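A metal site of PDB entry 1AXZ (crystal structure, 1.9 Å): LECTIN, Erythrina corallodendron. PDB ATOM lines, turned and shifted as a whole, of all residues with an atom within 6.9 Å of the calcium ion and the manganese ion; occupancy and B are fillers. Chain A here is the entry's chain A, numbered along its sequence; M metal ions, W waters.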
ATOM      1  N   ASP A  89      17.505   0.814  23.091  1.00  0.00           N
ATOM      2  CA  ASP A  89      16.442  -0.054  23.582  1.00  0.00           C
ATOM      3  C   ASP A  89      16.173   0.132  25.083  1.00  0.00           C
ATOM      4  O   ASP A  89      15.078  -0.179  25.555  1.00  0.00           O
ATOM      5  CB  ASP A  89      16.794  -1.524  23.328  1.00  0.00           C
ATOM      6  CG  ASP A  89      16.257  -2.029  22.009  1.00  0.00           C
ATOM      7  OD1 ASP A  89      15.038  -2.270  21.910  1.00  0.00           O
ATOM      8  OD2 ASP A  89      17.060  -2.186  21.074  1.00  0.00           O
ATOM      9  N   GLY A  90      17.185   0.574  25.811  1.00  0.00           N
ATOM     10  CA  GLY A  90      17.019   0.807  27.237  1.00  0.00           C
ATOM     11  C   GLY A  90      18.156   0.300  28.102  1.00  0.00           C
ATOM     12  O   GLY A  90      19.188  -0.132  27.591  1.00  0.00           O
ATOM     13  N   TYR A 106      19.635  -5.633  21.922  1.00  0.00           N
ATOM     14  CA  TYR A 106      18.365  -5.063  21.481  1.00  0.00           C
ATOM     15  C   TYR A 106      17.331  -5.080  22.614  1.00  0.00           C
ATOM     16  O   TYR A 106      17.651  -4.738  23.753  1.00  0.00           O
ATOM     17  CB  TYR A 106      17.834  -5.818  20.247  1.00  0.00           C
ATOM     18  CG  TYR A 106      18.883  -6.027  19.171  1.00  0.00           C
ATOM     19  CD1 TYR A 106      19.782  -5.016  18.833  1.00  0.00           C
ATOM     20  CD2 TYR A 106      18.990  -7.245  18.507  1.00  0.00           C
ATOM     21  CE1 TYR A 106      20.763  -5.211  17.875  1.00  0.00           C
ATOM     22  CE2 TYR A 106      19.966  -7.462  17.545  1.00  0.00           C
ATOM     23  CZ  TYR A 106      20.848  -6.438  17.230  1.00  0.00           C
ATOM     24  OH  TYR A 106      21.828  -6.651  16.290  1.00  0.00           O
ATOM     25  N   GLY A 107      16.099  -5.472  22.290  1.00  0.00           N
ATOM     26  CA  GLY A 107      15.036  -5.525  23.272  1.00  0.00           C
ATOM     27  C   GLY A 107      15.251  -6.472  24.443  1.00  0.00           C
ATOM     28  O   GLY A 107      14.509  -6.407  25.431  1.00  0.00           O
ATOM     29  N   TYR A 108      16.225  -7.362  24.330  1.00  0.00           N
ATOM     30  CA  TYR A 108      16.524  -8.314  25.405  1.00  0.00           C
ATOM     31  C   TYR A 108      17.444  -7.687  26.447  1.00  0.00           C
ATOM     32  O   TYR A 108      17.746  -8.281  27.477  1.00  0.00           O
ATOM     33  CB  TYR A 108      17.110  -9.604  24.842  1.00  0.00           C
ATOM     34  CG  TYR A 108      16.153 -10.273  23.883  1.00  0.00           C
ATOM     35  CD1 TYR A 108      14.911 -10.711  24.304  1.00  0.00           C
ATOM     36  CD2 TYR A 108      16.488 -10.417  22.529  1.00  0.00           C
ATOM     37  CE1 TYR A 108      13.999 -11.272  23.406  1.00  0.00           C
ATOM     38  CE2 TYR A 108      15.584 -10.981  21.635  1.00  0.00           C
ATOM     39  CZ  TYR A 108      14.341 -11.404  22.072  1.00  0.00           C
ATOM     40  OH  TYR A 108      13.445 -11.955  21.197  1.00  0.00           O
ATOM     41  N   LEU A 109      17.923  -6.487  26.126  1.00  0.00           N
ATOM     42  CA  LEU A 109      18.763  -5.685  27.012  1.00  0.00           C
ATOM     43  C   LEU A 109      20.079  -6.283  27.510  1.00  0.00           C
ATOM     44  O   LEU A 109      20.648  -5.798  28.491  1.00  0.00           O
ATOM     45  CB  LEU A 109      17.923  -5.213  28.206  1.00  0.00           C
ATOM     46  CG  LEU A 109      16.599  -4.525  27.827  1.00  0.00           C
ATOM     47  CD1 LEU A 109      15.775  -4.235  29.083  1.00  0.00           C
ATOM     48  CD2 LEU A 109      16.877  -3.239  27.050  1.00  0.00           C
ATOM     49  N   GLU A 127      14.015  -2.830  34.696  1.00  0.00           N
ATOM     50  CA  GLU A 127      14.340  -2.174  33.438  1.00  0.00           C
ATOM     51  C   GLU A 127      13.741  -0.791  33.266  1.00  0.00           C
ATOM     52  O   GLU A 127      12.736  -0.445  33.883  1.00  0.00           O
ATOM     53  CB  GLU A 127      13.856  -3.032  32.279  1.00  0.00           C
ATOM     54  CG  GLU A 127      12.367  -3.297  32.375  1.00  0.00           C
ATOM     55  CD  GLU A 127      11.780  -3.877  31.114  1.00  0.00           C
ATOM     56  OE1 GLU A 127      12.261  -4.919  30.649  1.00  0.00           O
ATOM     57  OE2 GLU A 127      10.835  -3.264  30.609  1.00  0.00           O
ATOM     58  N   PHE A 128      14.396  -0.030  32.386  1.00  0.00           N
ATOM     59  CA  PHE A 128      14.002   1.322  31.997  1.00  0.00           C
ATOM     60  C   PHE A 128      14.064   1.179  30.485  1.00  0.00           C
ATOM     61  O   PHE A 128      15.091   1.342  29.839  1.00  0.00           O
ATOM     62  CB  PHE A 128      15.009   2.331  32.566  1.00  0.00           C
ATOM     63  CG  PHE A 128      15.047   2.315  34.066  1.00  0.00           C
ATOM     64  CD1 PHE A 128      14.137   3.084  34.797  1.00  0.00           C
ATOM     65  CD2 PHE A 128      15.904   1.459  34.749  1.00  0.00           C
ATOM     66  CE1 PHE A 128      14.092   3.002  36.198  1.00  0.00           C
ATOM     67  CE2 PHE A 128      15.858   1.365  36.143  1.00  0.00           C
ATOM     68  CZ  PHE A 128      14.955   2.139  36.862  1.00  0.00           C
ATOM     69  N   ASP A 129      12.929   0.711  29.975  1.00  0.00           N
ATOM     70  CA  ASP A 129      12.709   0.385  28.582  1.00  0.00           C
ATOM     71  C   ASP A 129      12.207   1.533  27.718  1.00  0.00           C
ATOM     72  O   ASP A 129      11.126   2.067  27.965  1.00  0.00           O
ATOM     73  CB  ASP A 129      11.705  -0.748  28.559  1.00  0.00           C
ATOM     74  CG  ASP A 129      11.684  -1.486  27.257  1.00  0.00           C
ATOM     75  OD1 ASP A 129      12.157  -0.970  26.239  1.00  0.00           O
ATOM     76  OD2 ASP A 129      11.208  -2.616  27.275  1.00  0.00           O
ATOM     77  N   THR A 130      12.916   1.781  26.625  1.00  0.00           N
ATOM     78  CA  THR A 130      12.582   2.881  25.728  1.00  0.00           C
ATOM     79  C   THR A 130      11.947   2.524  24.381  1.00  0.00           C
ATOM     80  O   THR A 130      11.553   3.416  23.622  1.00  0.00           O
ATOM     81  CB  THR A 130      13.834   3.729  25.444  1.00  0.00           C
ATOM     82  OG1 THR A 130      14.857   2.891  24.905  1.00  0.00           O
ATOM     83  CG2 THR A 130      14.345   4.362  26.740  1.00  0.00           C
ATOM     84  N   PHE A 131      11.870   1.227  24.069  1.00  0.00           N
ATOM     85  CA  PHE A 131      11.284   0.800  22.796  1.00  0.00           C
ATOM     86  C   PHE A 131      10.221  -0.269  23.018  1.00  0.00           C
ATOM     87  O   PHE A 131      10.463  -1.255  23.713  1.00  0.00           O
ATOM     88  CB  PHE A 131      12.376   0.261  21.866  1.00  0.00           C
ATOM     89  CG  PHE A 131      11.859  -0.161  20.512  1.00  0.00           C
ATOM     90  CD1 PHE A 131      11.392  -1.458  20.319  1.00  0.00           C
ATOM     91  CD2 PHE A 131      11.819   0.738  19.455  1.00  0.00           C
ATOM     92  CE1 PHE A 131      10.881  -1.855  19.078  1.00  0.00           C
ATOM     93  CE2 PHE A 131      11.312   0.351  18.212  1.00  0.00           C
ATOM     94  CZ  PHE A 131      10.842  -0.944  18.028  1.00  0.00           C
ATOM     95  N   SER A 132       9.058  -0.101  22.406  1.00  0.00           N
ATOM     96  CA  SER A 132       7.980  -1.075  22.577  1.00  0.00           C
ATOM     97  C   SER A 132       8.075  -2.285  21.652  1.00  0.00           C
ATOM     98  O   SER A 132       7.781  -2.184  20.455  1.00  0.00           O
ATOM     99  CB  SER A 132       6.611  -0.394  22.409  1.00  0.00           C
ATOM    100  OG  SER A 132       5.566  -1.284  22.759  1.00  0.00           O
ATOM    101  N   ASN A 133       8.526  -3.412  22.195  1.00  0.00           N
ATOM    102  CA  ASN A 133       8.633  -4.660  21.454  1.00  0.00           C
ATOM    103  C   ASN A 133       7.262  -5.347  21.499  1.00  0.00           C
ATOM    104  O   ASN A 133       6.364  -4.881  22.203  1.00  0.00           O
ATOM    105  CB  ASN A 133       9.701  -5.565  22.083  1.00  0.00           C
ATOM    106  CG  ASN A 133      11.100  -4.992  21.989  1.00  0.00           C
ATOM    107  OD1 ASN A 133      11.574  -4.337  22.901  1.00  0.00           O
ATOM    108  ND2 ASN A 133      11.769  -5.236  20.870  1.00  0.00           N
ATOM    109  N   TRP A 135       6.235  -7.859  23.059  1.00  0.00           N
ATOM    110  CA  TRP A 135       5.910  -8.336  24.405  1.00  0.00           C
ATOM    111  C   TRP A 135       5.725  -7.183  25.392  1.00  0.00           C
ATOM    112  O   TRP A 135       5.456  -7.402  26.568  1.00  0.00           O
ATOM    113  CB  TRP A 135       7.021  -9.255  24.919  1.00  0.00           C
ATOM    114  CG  TRP A 135       8.382  -8.621  24.913  1.00  0.00           C
ATOM    115  CD1 TRP A 135       8.888  -7.733  25.824  1.00  0.00           C
ATOM    116  CD2 TRP A 135       9.409  -8.808  23.932  1.00  0.00           C
ATOM    117  NE1 TRP A 135      10.164  -7.371  25.475  1.00  0.00           N
ATOM    118  CE2 TRP A 135      10.520  -8.024  24.317  1.00  0.00           C
ATOM    119  CE3 TRP A 135       9.509  -9.587  22.770  1.00  0.00           C
ATOM    120  CZ2 TRP A 135      11.705  -7.975  23.582  1.00  0.00           C
ATOM    121  CZ3 TRP A 135      10.694  -9.537  22.035  1.00  0.00           C
ATOM    122  CH2 TRP A 135      11.777  -8.734  22.449  1.00  0.00           C
ATOM    123  N   ASP A 136       5.899  -5.960  24.896  1.00  0.00           N
ATOM    124  CA  ASP A 136       5.786  -4.749  25.704  1.00  0.00           C
ATOM    125  C   ASP A 136       4.449  -4.051  25.661  1.00  0.00           C
ATOM    126  O   ASP A 136       3.664  -4.240  24.728  1.00  0.00           O
ATOM    127  CB  ASP A 136       6.808  -3.713  25.227  1.00  0.00           C
ATOM    128  CG  ASP A 136       8.188  -3.996  25.714  1.00  0.00           C
ATOM    129  OD1 ASP A 136       8.300  -4.522  26.818  1.00  0.00           O
ATOM    130  OD2 ASP A 136       9.157  -3.724  24.998  1.00  0.00           O
ATOM    131  N   PRO A 137       4.148  -3.249  26.701  1.00  0.00           N
ATOM    132  CA  PRO A 137       2.894  -2.508  26.710  1.00  0.00           C
ATOM    133  C   PRO A 137       3.181  -1.396  25.691  1.00  0.00           C
ATOM    134  O   PRO A 137       4.350  -1.091  25.420  1.00  0.00           O
ATOM    135  CB  PRO A 137       2.833  -1.961  28.137  1.00  0.00           C
ATOM    136  CG  PRO A 137       4.278  -1.838  28.524  1.00  0.00           C
ATOM    137  CD  PRO A 137       4.856  -3.118  27.988  1.00  0.00           C
ATOM    138  N   VAL A 140       5.896   3.810  26.161  1.00  0.00           N
ATOM    139  CA  VAL A 140       7.337   3.882  26.378  1.00  0.00           C
ATOM    140  C   VAL A 140       7.730   5.343  26.554  1.00  0.00           C
ATOM    141  O   VAL A 140       7.125   6.237  25.976  1.00  0.00           O
ATOM    142  CB  VAL A 140       8.172   3.263  25.215  1.00  0.00           C
ATOM    143  CG1 VAL A 140       8.087   1.745  25.261  1.00  0.00           C
ATOM    144  CG2 VAL A 140       7.690   3.801  23.865  1.00  0.00           C
ATOM    145  N   HIS A 142       9.098   2.978  29.966  1.00  0.00           N
ATOM    146  CA  HIS A 142       8.448   2.434  31.142  1.00  0.00           C
ATOM    147  C   HIS A 142       9.428   1.671  32.013  1.00  0.00           C
ATOM    148  O   HIS A 142      10.471   1.189  31.546  1.00  0.00           O
ATOM    149  CB  HIS A 142       7.267   1.527  30.771  1.00  0.00           C
ATOM    150  CG  HIS A 142       7.629   0.377  29.880  1.00  0.00           C
ATOM    151  ND1 HIS A 142       7.407   0.363  28.525  1.00  0.00           N
ATOM    152  CD2 HIS A 142       8.217  -0.815  30.177  1.00  0.00           C
ATOM    153  CE1 HIS A 142       7.857  -0.811  28.055  1.00  0.00           C
ATOM    154  NE2 HIS A 142       8.349  -1.547  29.029  1.00  0.00           N
ATOM    155  N   ILE A 143       9.126   1.663  33.301  1.00  0.00           N
ATOM    156  CA  ILE A 143       9.916   0.930  34.271  1.00  0.00           C
ATOM    157  C   ILE A 143       9.238  -0.425  34.293  1.00  0.00           C
ATOM    158  O   ILE A 143       8.013  -0.513  34.167  1.00  0.00           O
ATOM    159  CB  ILE A 143       9.793   1.525  35.695  1.00  0.00           C
ATOM    160  CG1 ILE A 143      10.121   3.021  35.673  1.00  0.00           C
ATOM    161  CG2 ILE A 143      10.734   0.791  36.655  1.00  0.00           C
ATOM    162  CD1 ILE A 143       9.821   3.735  36.990  1.00  0.00           C
ATOM    163  N   GLY A 144      10.017  -1.494  34.423  1.00  0.00           N
ATOM    164  CA  GLY A 144       9.421  -2.812  34.466  1.00  0.00           C
ATOM    165  C   GLY A 144      10.175  -3.727  35.405  1.00  0.00           C
ATOM    166  O   GLY A 144      11.385  -3.601  35.568  1.00  0.00           O
ATOM    167  N   ASP A 146      11.260  -7.393  35.900  1.00  0.00           N
ATOM    168  CA  ASP A 146      11.445  -8.616  35.128  1.00  0.00           C
ATOM    169  C   ASP A 146      11.872  -9.787  35.990  1.00  0.00           C
ATOM    170  O   ASP A 146      12.922  -9.753  36.628  1.00  0.00           O
ATOM    171  CB  ASP A 146      12.507  -8.385  34.045  1.00  0.00           C
ATOM    172  CG  ASP A 146      12.181  -7.229  33.118  1.00  0.00           C
ATOM    173  OD1 ASP A 146      11.032  -6.745  33.133  1.00  0.00           O
ATOM    174  OD2 ASP A 146      13.084  -6.791  32.366  1.00  0.00           O
ATOM    175  N   ILE A 150      11.804 -11.208  29.882  1.00  0.00           N
ATOM    176  CA  ILE A 150      11.808  -9.830  29.400  1.00  0.00           C
ATOM    177  C   ILE A 150      10.360  -9.318  29.450  1.00  0.00           C
ATOM    178  O   ILE A 150      10.106  -8.116  29.335  1.00  0.00           O
ATOM    179  CB  ILE A 150      12.408  -9.750  27.974  1.00  0.00           C
ATOM    180  CG1 ILE A 150      12.709  -8.294  27.605  1.00  0.00           C
ATOM    181  CG2 ILE A 150      11.478 -10.412  26.953  1.00  0.00           C
ATOM    182  CD1 ILE A 150      13.781  -7.651  28.485  1.00  0.00           C
ATOM    183  N   ARG A 151       9.417 -10.242  29.609  1.00  0.00           N
ATOM    184  CA  ARG A 151       8.003  -9.901  29.710  1.00  0.00           C
ATOM    185  C   ARG A 151       7.721  -9.562  31.173  1.00  0.00           C
ATOM    186  O   ARG A 151       7.398 -10.443  31.973  1.00  0.00           O
ATOM    187  CB  ARG A 151       7.125 -11.081  29.265  1.00  0.00           C
ATOM    188  CG  ARG A 151       7.188 -11.365  27.773  1.00  0.00           C
ATOM    189  CD  ARG A 151       6.135 -12.383  27.360  1.00  0.00           C
ATOM    190  NE  ARG A 151       6.666 -13.740  27.337  1.00  0.00           N
ATOM    191  CZ  ARG A 151       6.155 -14.772  28.006  1.00  0.00           C
ATOM    192  NH1 ARG A 151       5.081 -14.617  28.774  1.00  0.00           N
ATOM    193  NH2 ARG A 151       6.711 -15.961  27.894  1.00  0.00           N
ATOM    194  N   SER A 152       7.821  -8.283  31.498  1.00  0.00           N
ATOM    195  CA  SER A 152       7.642  -7.789  32.865  1.00  0.00           C
ATOM    196  C   SER A 152       6.356  -8.232  33.553  1.00  0.00           C
ATOM    197  O   SER A 152       5.303  -8.329  32.927  1.00  0.00           O
ATOM    198  CB  SER A 152       7.692  -6.262  32.884  1.00  0.00           C
ATOM    199  OG  SER A 152       8.845  -5.778  32.220  1.00  0.00           O
ATOM    200  N   THR A 155       4.594  -3.118  35.052  1.00  0.00           N
ATOM    201  CA  THR A 155       5.169  -1.999  34.302  1.00  0.00           C
ATOM    202  C   THR A 155       4.602  -0.666  34.800  1.00  0.00           C
ATOM    203  O   THR A 155       3.495  -0.617  35.344  1.00  0.00           O
ATOM    204  CB  THR A 155       4.868  -2.154  32.778  1.00  0.00           C
ATOM    205  OG1 THR A 155       5.764  -3.134  32.211  1.00  0.00           O
ATOM    206  CG2 THR A 155       5.045  -0.859  32.035  1.00  0.00           C
HETATM  207 CA    CA M   1      11.468  -3.055  24.914  1.00  0.00          CA
HETATM  208 MN    MN M   2       9.548  -3.633  28.644  1.00  0.00          MN
HETATM  209  O   HOH W   1      12.270  -5.073  26.048  1.00  0.00           O
HETATM  210  O   HOH W   2      13.703  -2.363  24.245  1.00  0.00           O
HETATM  211  O   HOH W   3      10.876  -5.738  28.503  1.00  0.00           O
HETATM  212  O   HOH W   4       7.855  -4.757  29.976  1.00  0.00           O
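Within 4 Å of the calcium ion: Asp 129, Phe 131, Asn 133 and Asp 136. The nearest printed residue that does not touch the calcium ion is Trp 135 (4.5 Å).
OE1 of Glu 127 sits close to OD2 of Asp 146. The backbone carbonyl oxygen (O) of Gly 144 sits at hydrogen-bond distance from the backbone NH (N) of Glu 127.
The calcium ion is bound by O of Phe 131. The calcium ion is bound by OD1 of Asn 133 (2.4 Å). The calcium ion is bound by OD2 of Asp 136, 2.4 Å away. The side-chain carboxylate (OD2) of Asp 129 binds the calcium ion, at 2.4 Å. The calcium ion is bound by water W2 (2.4 Å). Water W1 is bound to the calcium ion (2.4 Å). The calcium ion is bound by OD1 of Asp 129.
The manganese ion is bound by OE2 of Glu 127 (2.4 Å), OD2 of Asp 129 (2.4 Å), OD1 of Asp 136 (2.4 Å), water W4 (2.4 Å), NE2 of His 142 (2.4 Å) and water W3 (2.5 Å). The manganese ion has six donor atoms within binding distance.
Within 4 Å of the manganese ion: Glu 127, Asp 129, Asp 136 and His 142.
Water W1 lies within hydrogen-bond range of O of Gly 107 and NE1 of Trp 135. Water W3 lies within hydrogen-bond range of the backbone carbonyl oxygen (O) of Ile 150 and the side-chain carboxylate (OE1) of Glu 127. Water W4 bridges OG of Ser 152 (2.7 Å) and OG1 of Thr 155 (3.5 Å).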
